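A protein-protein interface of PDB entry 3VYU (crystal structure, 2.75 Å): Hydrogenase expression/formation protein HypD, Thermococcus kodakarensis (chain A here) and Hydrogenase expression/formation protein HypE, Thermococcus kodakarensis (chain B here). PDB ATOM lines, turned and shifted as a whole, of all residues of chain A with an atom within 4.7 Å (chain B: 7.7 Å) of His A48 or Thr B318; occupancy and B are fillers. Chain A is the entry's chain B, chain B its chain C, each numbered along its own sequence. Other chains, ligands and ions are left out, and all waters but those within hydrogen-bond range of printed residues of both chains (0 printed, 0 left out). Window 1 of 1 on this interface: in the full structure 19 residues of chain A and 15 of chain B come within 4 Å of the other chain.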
ATOM      1  N   ASP A  43      11.324 -12.492   3.619  1.00  0.00           N
ATOM      2  CA  ASP A  43      11.451 -12.316   5.060  1.00  0.00           C
ATOM      3  C   ASP A  43      12.925 -12.314   5.453  1.00  0.00           C
ATOM      4  O   ASP A  43      13.348 -11.509   6.283  1.00  0.00           O
ATOM      5  CB  ASP A  43      10.702 -13.428   5.805  1.00  0.00           C
ATOM      6  CG  ASP A  43      10.630 -13.185   7.311  1.00  0.00           C
ATOM      7  OD1 ASP A  43      11.687 -13.246   7.977  1.00  0.00           O
ATOM      8  OD2 ASP A  43       9.517 -12.935   7.830  1.00  0.00           O
ATOM      9  N   THR A  44      13.711 -13.203   4.851  1.00  0.00           N
ATOM     10  CA  THR A  44      15.139 -13.267   5.155  1.00  0.00           C
ATOM     11  C   THR A  44      15.837 -11.957   4.795  1.00  0.00           C
ATOM     12  O   THR A  44      16.574 -11.394   5.609  1.00  0.00           O
ATOM     13  CB  THR A  44      15.827 -14.411   4.390  1.00  0.00           C
ATOM     14  OG1 THR A  44      15.332 -15.665   4.866  1.00  0.00           O
ATOM     15  CG2 THR A  44      17.328 -14.360   4.589  1.00  0.00           C
ATOM     16  N   VAL A  45      15.595 -11.481   3.576  1.00  0.00           N
ATOM     17  CA  VAL A  45      16.192 -10.244   3.082  1.00  0.00           C
ATOM     18  C   VAL A  45      15.801  -9.035   3.923  1.00  0.00           C
ATOM     19  O   VAL A  45      16.642  -8.195   4.251  1.00  0.00           O
ATOM     20  CB  VAL A  45      15.763  -9.959   1.632  1.00  0.00           C
ATOM     21  CG1 VAL A  45      16.327  -8.625   1.175  1.00  0.00           C
ATOM     22  CG2 VAL A  45      16.233 -11.070   0.725  1.00  0.00           C
ATOM     23  N   THR A  46      14.519  -8.948   4.261  1.00  0.00           N
ATOM     24  CA  THR A  46      14.014  -7.835   5.046  1.00  0.00           C
ATOM     25  C   THR A  46      14.364  -7.918   6.530  1.00  0.00           C
ATOM     26  O   THR A  46      14.732  -6.905   7.131  1.00  0.00           O
ATOM     27  CB  THR A  46      12.487  -7.697   4.886  1.00  0.00           C
ATOM     28  OG1 THR A  46      12.187  -7.291   3.544  1.00  0.00           O
ATOM     29  CG2 THR A  46      11.940  -6.666   5.852  1.00  0.00           C
ATOM     30  N   ARG A  47      14.259  -9.111   7.119  1.00  0.00           N
ATOM     31  CA  ARG A  47      14.571  -9.283   8.541  1.00  0.00           C
ATOM     32  C   ARG A  47      16.011  -8.908   8.860  1.00  0.00           C
ATOM     33  O   ARG A  47      16.275  -8.213   9.842  1.00  0.00           O
ATOM     34  CB  ARG A  47      14.346 -10.719   9.008  1.00  0.00           C
ATOM     35  CG  ARG A  47      14.648 -10.887  10.497  1.00  0.00           C
ATOM     36  CD  ARG A  47      14.836 -12.338  10.915  1.00  0.00           C
ATOM     37  NE  ARG A  47      13.707 -13.181  10.543  1.00  0.00           N
ATOM     38  CZ  ARG A  47      13.335 -14.259  11.222  1.00  0.00           C
ATOM     39  NH1 ARG A  47      14.004 -14.616  12.311  1.00  0.00           N
ATOM     40  NH2 ARG A  47      12.297 -14.979  10.815  1.00  0.00           N
ATOM     41  N   HIS A  48      16.945  -9.382   8.045  1.00  0.00           N
ATOM     42  CA  HIS A  48      18.344  -9.054   8.274  1.00  0.00           C
ATOM     43  C   HIS A  48      18.736  -7.773   7.535  1.00  0.00           C
ATOM     44  O   HIS A  48      19.901  -7.374   7.542  1.00  0.00           O
ATOM     45  CB  HIS A  48      19.236 -10.219   7.836  1.00  0.00           C
ATOM     46  CG  HIS A  48      18.930 -11.497   8.544  1.00  0.00           C
ATOM     47  ND1 HIS A  48      18.177 -12.516   7.974  1.00  0.00           N
ATOM     48  CD2 HIS A  48      19.248 -11.925   9.782  1.00  0.00           C
ATOM     49  CE1 HIS A  48      18.059 -13.500   8.834  1.00  0.00           C
ATOM     50  NE2 HIS A  48      18.700 -13.172   9.948  1.00  0.00           N
ATOM     51  N   GLY A  49      17.757  -7.138   6.894  1.00  0.00           N
ATOM     52  CA  GLY A  49      18.020  -5.911   6.155  1.00  0.00           C
ATOM     53  C   GLY A  49      19.181  -6.026   5.182  1.00  0.00           C
ATOM     54  O   GLY A  49      20.092  -5.197   5.171  1.00  0.00           O
ATOM     55  N   ILE A  50      19.148  -7.065   4.359  1.00  0.00           N
ATOM     56  CA  ILE A  50      20.202  -7.281   3.386  1.00  0.00           C
ATOM     57  C   ILE A  50      20.225  -6.138   2.388  1.00  0.00           C
ATOM     58  O   ILE A  50      21.296  -5.685   1.988  1.00  0.00           O
ATOM     59  CB  ILE A  50      20.015  -8.631   2.651  1.00  0.00           C
ATOM     60  CG1 ILE A  50      20.358  -9.782   3.600  1.00  0.00           C
ATOM     61  CG2 ILE A  50      20.897  -8.692   1.422  1.00  0.00           C
ATOM     62  CD1 ILE A  50      20.124 -11.149   3.023  1.00  0.00           C
ATOM     63  N   PRO A 230      20.784 -15.801   6.300  1.00  0.00           N
ATOM     64  CA  PRO A 230      21.199 -14.544   5.668  1.00  0.00           C
ATOM     65  C   PRO A 230      22.363 -14.717   4.697  1.00  0.00           C
ATOM     66  O   PRO A 230      22.419 -14.062   3.654  1.00  0.00           O
ATOM     67  CB  PRO A 230      21.555 -13.654   6.859  1.00  0.00           C
ATOM     68  CG  PRO A 230      21.957 -14.643   7.923  1.00  0.00           C
ATOM     69  CD  PRO A 230      20.918 -15.722   7.764  1.00  0.00           C
ATOM     70  N   LEU B 243      19.546   3.308  19.012  1.00  0.00           N
ATOM     71  CA  LEU B 243      20.195   2.273  18.218  1.00  0.00           C
ATOM     72  C   LEU B 243      20.434   1.021  19.058  1.00  0.00           C
ATOM     73  O   LEU B 243      21.073   1.070  20.111  1.00  0.00           O
ATOM     74  CB  LEU B 243      21.522   2.795  17.657  1.00  0.00           C
ATOM     75  CG  LEU B 243      22.396   1.806  16.879  1.00  0.00           C
ATOM     76  CD1 LEU B 243      21.597   1.160  15.757  1.00  0.00           C
ATOM     77  CD2 LEU B 243      23.607   2.540  16.323  1.00  0.00           C
ATOM     78  N   VAL B 244      19.908  -0.100  18.584  1.00  0.00           N
ATOM     79  CA  VAL B 244      20.049  -1.367  19.281  1.00  0.00           C
ATOM     80  C   VAL B 244      20.745  -2.388  18.397  1.00  0.00           C
ATOM     81  O   VAL B 244      20.454  -2.495  17.206  1.00  0.00           O
ATOM     82  CB  VAL B 244      18.674  -1.916  19.699  1.00  0.00           C
ATOM     83  CG1 VAL B 244      18.814  -3.318  20.252  1.00  0.00           C
ATOM     84  CG2 VAL B 244      18.061  -1.008  20.741  1.00  0.00           C
ATOM     85  N   ARG B 245      21.665  -3.141  18.990  1.00  0.00           N
ATOM     86  CA  ARG B 245      22.412  -4.160  18.266  1.00  0.00           C
ATOM     87  C   ARG B 245      21.844  -5.542  18.554  1.00  0.00           C
ATOM     88  O   ARG B 245      21.977  -6.070  19.657  1.00  0.00           O
ATOM     89  CB  ARG B 245      23.888  -4.064  18.650  1.00  0.00           C
ATOM     90  CG  ARG B 245      24.459  -2.702  18.275  1.00  0.00           C
ATOM     91  CD  ARG B 245      25.725  -2.328  19.027  1.00  0.00           C
ATOM     92  NE  ARG B 245      25.867  -0.872  19.083  1.00  0.00           N
ATOM     93  CZ  ARG B 245      26.030  -0.087  18.020  1.00  0.00           C
ATOM     94  NH1 ARG B 245      26.084  -0.608  16.800  1.00  0.00           N
ATOM     95  NH2 ARG B 245      26.113   1.228  18.176  1.00  0.00           N
ATOM     96  N   GLU B 246      21.195  -6.110  17.542  1.00  0.00           N
ATOM     97  CA  GLU B 246      20.557  -7.418  17.632  1.00  0.00           C
ATOM     98  C   GLU B 246      21.463  -8.456  18.280  1.00  0.00           C
ATOM     99  O   GLU B 246      20.995  -9.350  18.988  1.00  0.00           O
ATOM    100  CB  GLU B 246      20.155  -7.884  16.231  1.00  0.00           C
ATOM    101  CG  GLU B 246      18.871  -8.694  16.180  1.00  0.00           C
ATOM    102  CD  GLU B 246      18.463  -9.053  14.760  1.00  0.00           C
ATOM    103  OE1 GLU B 246      19.237  -9.763  14.084  1.00  0.00           O
ATOM    104  OE2 GLU B 246      17.372  -8.627  14.318  1.00  0.00           O
ATOM    105  N   ALA B 247      22.761  -8.317  18.036  1.00  0.00           N
ATOM    106  CA  ALA B 247      23.757  -9.237  18.570  1.00  0.00           C
ATOM    107  C   ALA B 247      23.977  -9.105  20.077  1.00  0.00           C
ATOM    108  O   ALA B 247      24.538 -10.005  20.703  1.00  0.00           O
ATOM    109  CB  ALA B 247      25.079  -9.037  17.834  1.00  0.00           C
ATOM    110  N   GLU B 260      10.684 -18.646  16.752  1.00  0.00           N
ATOM    111  CA  GLU B 260      10.708 -18.970  15.327  1.00  0.00           C
ATOM    112  C   GLU B 260       9.544 -19.875  14.935  1.00  0.00           C
ATOM    113  O   GLU B 260       8.934 -19.700  13.880  1.00  0.00           O
ATOM    114  CB  GLU B 260      12.023 -19.669  14.973  1.00  0.00           C
ATOM    115  CG  GLU B 260      13.293 -18.847  15.222  1.00  0.00           C
ATOM    116  CD  GLU B 260      13.706 -17.976  14.037  1.00  0.00           C
ATOM    117  OE1 GLU B 260      14.646 -17.167  14.200  1.00  0.00           O
ATOM    118  OE2 GLU B 260      13.105 -18.101  12.946  1.00  0.00           O
ATOM    119  N   TYR B 267      11.180  -9.923  20.591  1.00  0.00           N
ATOM    120  CA  TYR B 267      11.217  -8.508  20.950  1.00  0.00           C
ATOM    121  C   TYR B 267       9.825  -7.966  21.240  1.00  0.00           C
ATOM    122  O   TYR B 267       9.670  -7.040  22.040  1.00  0.00           O
ATOM    123  CB  TYR B 267      11.844  -7.661  19.838  1.00  0.00           C
ATOM    124  CG  TYR B 267      13.219  -8.104  19.411  1.00  0.00           C
ATOM    125  CD1 TYR B 267      14.129  -8.609  20.335  1.00  0.00           C
ATOM    126  CD2 TYR B 267      13.609  -8.032  18.077  1.00  0.00           C
ATOM    127  CE1 TYR B 267      15.391  -9.038  19.940  1.00  0.00           C
ATOM    128  CE2 TYR B 267      14.869  -8.455  17.673  1.00  0.00           C
ATOM    129  CZ  TYR B 267      15.751  -8.959  18.608  1.00  0.00           C
ATOM    130  OH  TYR B 267      16.988  -9.402  18.210  1.00  0.00           O
ATOM    131  N   LEU B 315      16.135   2.149  15.878  1.00  0.00           N
ATOM    132  CA  LEU B 315      16.893   1.550  14.789  1.00  0.00           C
ATOM    133  C   LEU B 315      17.643   0.312  15.262  1.00  0.00           C
ATOM    134  O   LEU B 315      18.392   0.368  16.234  1.00  0.00           O
ATOM    135  CB  LEU B 315      17.872   2.585  14.236  1.00  0.00           C
ATOM    136  CG  LEU B 315      18.420   2.388  12.826  1.00  0.00           C
ATOM    137  CD1 LEU B 315      17.276   2.339  11.827  1.00  0.00           C
ATOM    138  CD2 LEU B 315      19.358   3.534  12.496  1.00  0.00           C
ATOM    139  N   LEU B 316      17.443  -0.802  14.565  1.00  0.00           N
ATOM    140  CA  LEU B 316      18.090  -2.057  14.920  1.00  0.00           C
ATOM    141  C   LEU B 316      19.161  -2.501  13.931  1.00  0.00           C
ATOM    142  O   LEU B 316      18.898  -2.638  12.737  1.00  0.00           O
ATOM    143  CB  LEU B 316      17.047  -3.167  15.041  1.00  0.00           C
ATOM    144  CG  LEU B 316      17.607  -4.590  15.157  1.00  0.00           C
ATOM    145  CD1 LEU B 316      18.331  -4.743  16.476  1.00  0.00           C
ATOM    146  CD2 LEU B 316      16.484  -5.604  15.057  1.00  0.00           C
ATOM    147  N   GLU B 317      20.370  -2.733  14.436  1.00  0.00           N
ATOM    148  CA  GLU B 317      21.467  -3.194  13.595  1.00  0.00           C
ATOM    149  C   GLU B 317      21.512  -4.713  13.725  1.00  0.00           C
ATOM    150  O   GLU B 317      21.953  -5.253  14.741  1.00  0.00           O
ATOM    151  CB  GLU B 317      22.804  -2.594  14.048  1.00  0.00           C
ATOM    152  CG  GLU B 317      23.890  -2.652  12.972  1.00  0.00           C
ATOM    153  CD  GLU B 317      25.280  -2.285  13.482  1.00  0.00           C
ATOM    154  OE1 GLU B 317      26.192  -2.111  12.644  1.00  0.00           O
ATOM    155  OE2 GLU B 317      25.468  -2.182  14.713  1.00  0.00           O
ATOM    156  N   THR B 318      21.037  -5.394  12.688  1.00  0.00           N
ATOM    157  CA  THR B 318      20.999  -6.850  12.666  1.00  0.00           C
ATOM    158  C   THR B 318      22.367  -7.495  12.855  1.00  0.00           C
ATOM    159  O   THR B 318      23.403  -6.841  12.721  1.00  0.00           O
ATOM    160  CB  THR B 318      20.401  -7.358  11.348  1.00  0.00           C
ATOM    161  OG1 THR B 318      21.139  -6.812  10.247  1.00  0.00           O
ATOM    162  CG2 THR B 318      18.944  -6.939  11.235  1.00  0.00           C
ATOM    163  N   GLY B 319      22.358  -8.790  13.157  1.00  0.00           N
ATOM    164  CA  GLY B 319      23.595  -9.517  13.376  1.00  0.00           C
ATOM    165  C   GLY B 319      24.601  -9.432  12.245  1.00  0.00           C
ATOM    166  O   GLY B 319      25.808  -9.379  12.491  1.00  0.00           O
ATOM    167  N   ILE B 320      24.114  -9.411  11.007  1.00  0.00           N
ATOM    168  CA  ILE B 320      24.997  -9.353   9.849  1.00  0.00           C
ATOM    169  C   ILE B 320      25.444  -7.937   9.465  1.00  0.00           C
ATOM    170  O   ILE B 320      26.081  -7.739   8.431  1.00  0.00           O
ATOM    171  CB  ILE B 320      24.336 -10.026   8.617  1.00  0.00           C
ATOM    172  CG1 ILE B 320      23.164  -9.182   8.108  1.00  0.00           C
ATOM    173  CG2 ILE B 320      23.829 -11.412   9.000  1.00  0.00           C
ATOM    174  CD1 ILE B 320      22.656  -9.608   6.737  1.00  0.00           C
ATOM    175  N   GLY B 321      25.117  -6.957  10.298  1.00  0.00           N
ATOM    176  CA  GLY B 321      25.511  -5.591  10.004  1.00  0.00           C
ATOM    177  C   GLY B 321      24.445  -4.786   9.284  1.00  0.00           C
ATOM    178  O   GLY B 321      24.638  -3.603   9.007  1.00  0.00           O
ATOM    179  N   GLY B 322      23.319  -5.423   8.980  1.00  0.00           N
ATOM    180  CA  GLY B 322      22.246  -4.728   8.294  1.00  0.00           C
ATOM    181  C   GLY B 322      21.492  -3.804   9.230  1.00  0.00           C
ATOM    182  O   GLY B 322      21.714  -3.825  10.441  1.00  0.00           O
ATOM    183  N   LYS B 323      20.602  -2.988   8.672  1.00  0.00           N
ATOM    184  CA  LYS B 323      19.816  -2.059   9.474  1.00  0.00           C
ATOM    185  C   LYS B 323      18.348  -1.994   9.068  1.00  0.00           C
ATOM    186  O   LYS B 323      18.010  -2.030   7.885  1.00  0.00           O
ATOM    187  CB  LYS B 323      20.415  -0.654   9.406  1.00  0.00           C
ATOM    188  CG  LYS B 323      21.539  -0.405  10.393  1.00  0.00           C
ATOM    189  CD  LYS B 323      22.011   1.041  10.340  1.00  0.00           C
ATOM    190  CE  LYS B 323      22.968   1.350  11.481  1.00  0.00           C
ATOM    191  NZ  LYS B 323      24.110   0.395  11.520  1.00  0.00           N
ATOM    192  N   ARG B 324      17.483  -1.890  10.073  1.00  0.00           N
ATOM    193  CA  ARG B 324      16.042  -1.804   9.873  1.00  0.00           C
ATOM    194  C   ARG B 324      15.442  -1.260  11.161  1.00  0.00           C
ATOM    195  O   ARG B 324      16.084  -1.302  12.210  1.00  0.00           O
ATOM    196  CB  ARG B 324      15.453  -3.184   9.577  1.00  0.00           C
ATOM    197  CG  ARG B 324      15.435  -4.131  10.770  1.00  0.00           C
ATOM    198  CD  ARG B 324      14.966  -5.514  10.350  1.00  0.00           C
ATOM    199  NE  ARG B 324      14.935  -6.460  11.462  1.00  0.00           N
ATOM    200  CZ  ARG B 324      14.045  -6.430  12.447  1.00  0.00           C
ATOM    201  NH1 ARG B 324      13.102  -5.499  12.466  1.00  0.00           N
ATOM    202  NH2 ARG B 324      14.096  -7.337  13.410  1.00  0.00           N
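OE1 of Glu B260 lies within salt-bridge range of NH1 of Arg A47. The backbone carbonyl oxygen of Arg A47 is in hydrogen-bond range of the guanidinium group of Arg B324 (2.7 Å). O of His A48 lies within hydrogen-bond range of OG1 of Thr B318 (3.0 Å).
The guanidinium group (NH2) of Arg B324 lies within salt-bridge range of the side-chain carboxylate (OE2) of Glu B246, at 3.6 Å. The backbone NH (N) of Ile A50 lies within hydrogen-bond range of the backbone carbonyl oxygen (O) of Val A45. O of Thr A44 is in hydrogen-bond range of ND1 of His A48, at 3.1 Å. The side-chain carboxylate (OD1) of Asp A43 is in salt-bridge range of the guanidinium group (NE) of Arg A47 (3.3 Å). The backbone NH (N) of Leu B316 is in hydrogen-bond range of the backbone carbonyl oxygen (O) of Arg B324 (2.8 Å). N of Gly B322 is in hydrogen-bond range of OG1 of Thr B318 (2.9 Å).
His A48 touches just these residues of chain B: Thr B318, Ile B320 and Gly B322. Of chain A, only Arg A47 (3.3 Å) and His A48 (3.0 Å) come within 4 Å of Thr B318. Printed residues of chain A within 4 Å of Gly B322: His A48 (3.6 Å) and Gly A49 (3.8 Å). Printed residues of chain A within 4 Å of Ile B320: His A48, Ile A50 and Pro A230. Printed residues of chain B within 4 Å of Pro A230: Ile B320 (3.8 Å). Of the printed residues of chain A, Arg B324 touches Thr A46 and Arg A47. Of the printed residues of chain A, Glu B260 touches Arg A47. Gly B321 touches none of the printed residues of chain A. Glu B317 touches none of the printed residues of chain A. The nearest residue of chain B that does not touch His A48 is Lys B323 (4.6 Å). The nearest residue of chain A that does not touch Thr B318 is Gly A49 (4.5 Å). The nearest printed residue of chain B that does not touch Thr A46 is Thr B318 (5.9 Å).
Printed residues of chain B that touch a printed residue of chain A: Glu B260, Thr B318, Ile B320, Gly B322 and Arg B324. Hydrophobic or aromatic side chains of chain B that line the printed part of chain A: Ile B320. Along chain A the printed residues that touch a printed residue of chain B span positions 46 to 230.
Among the printed residues, pairs that only touch across the chains: Arg A47 with Thr B318, Thr A46 with Arg B324, His A48 with Gly B322, His A48 with Ile B320, Gly A49 with Gly B322, Pro A230 with Ile B320 and Ile A50 with Ile B320.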
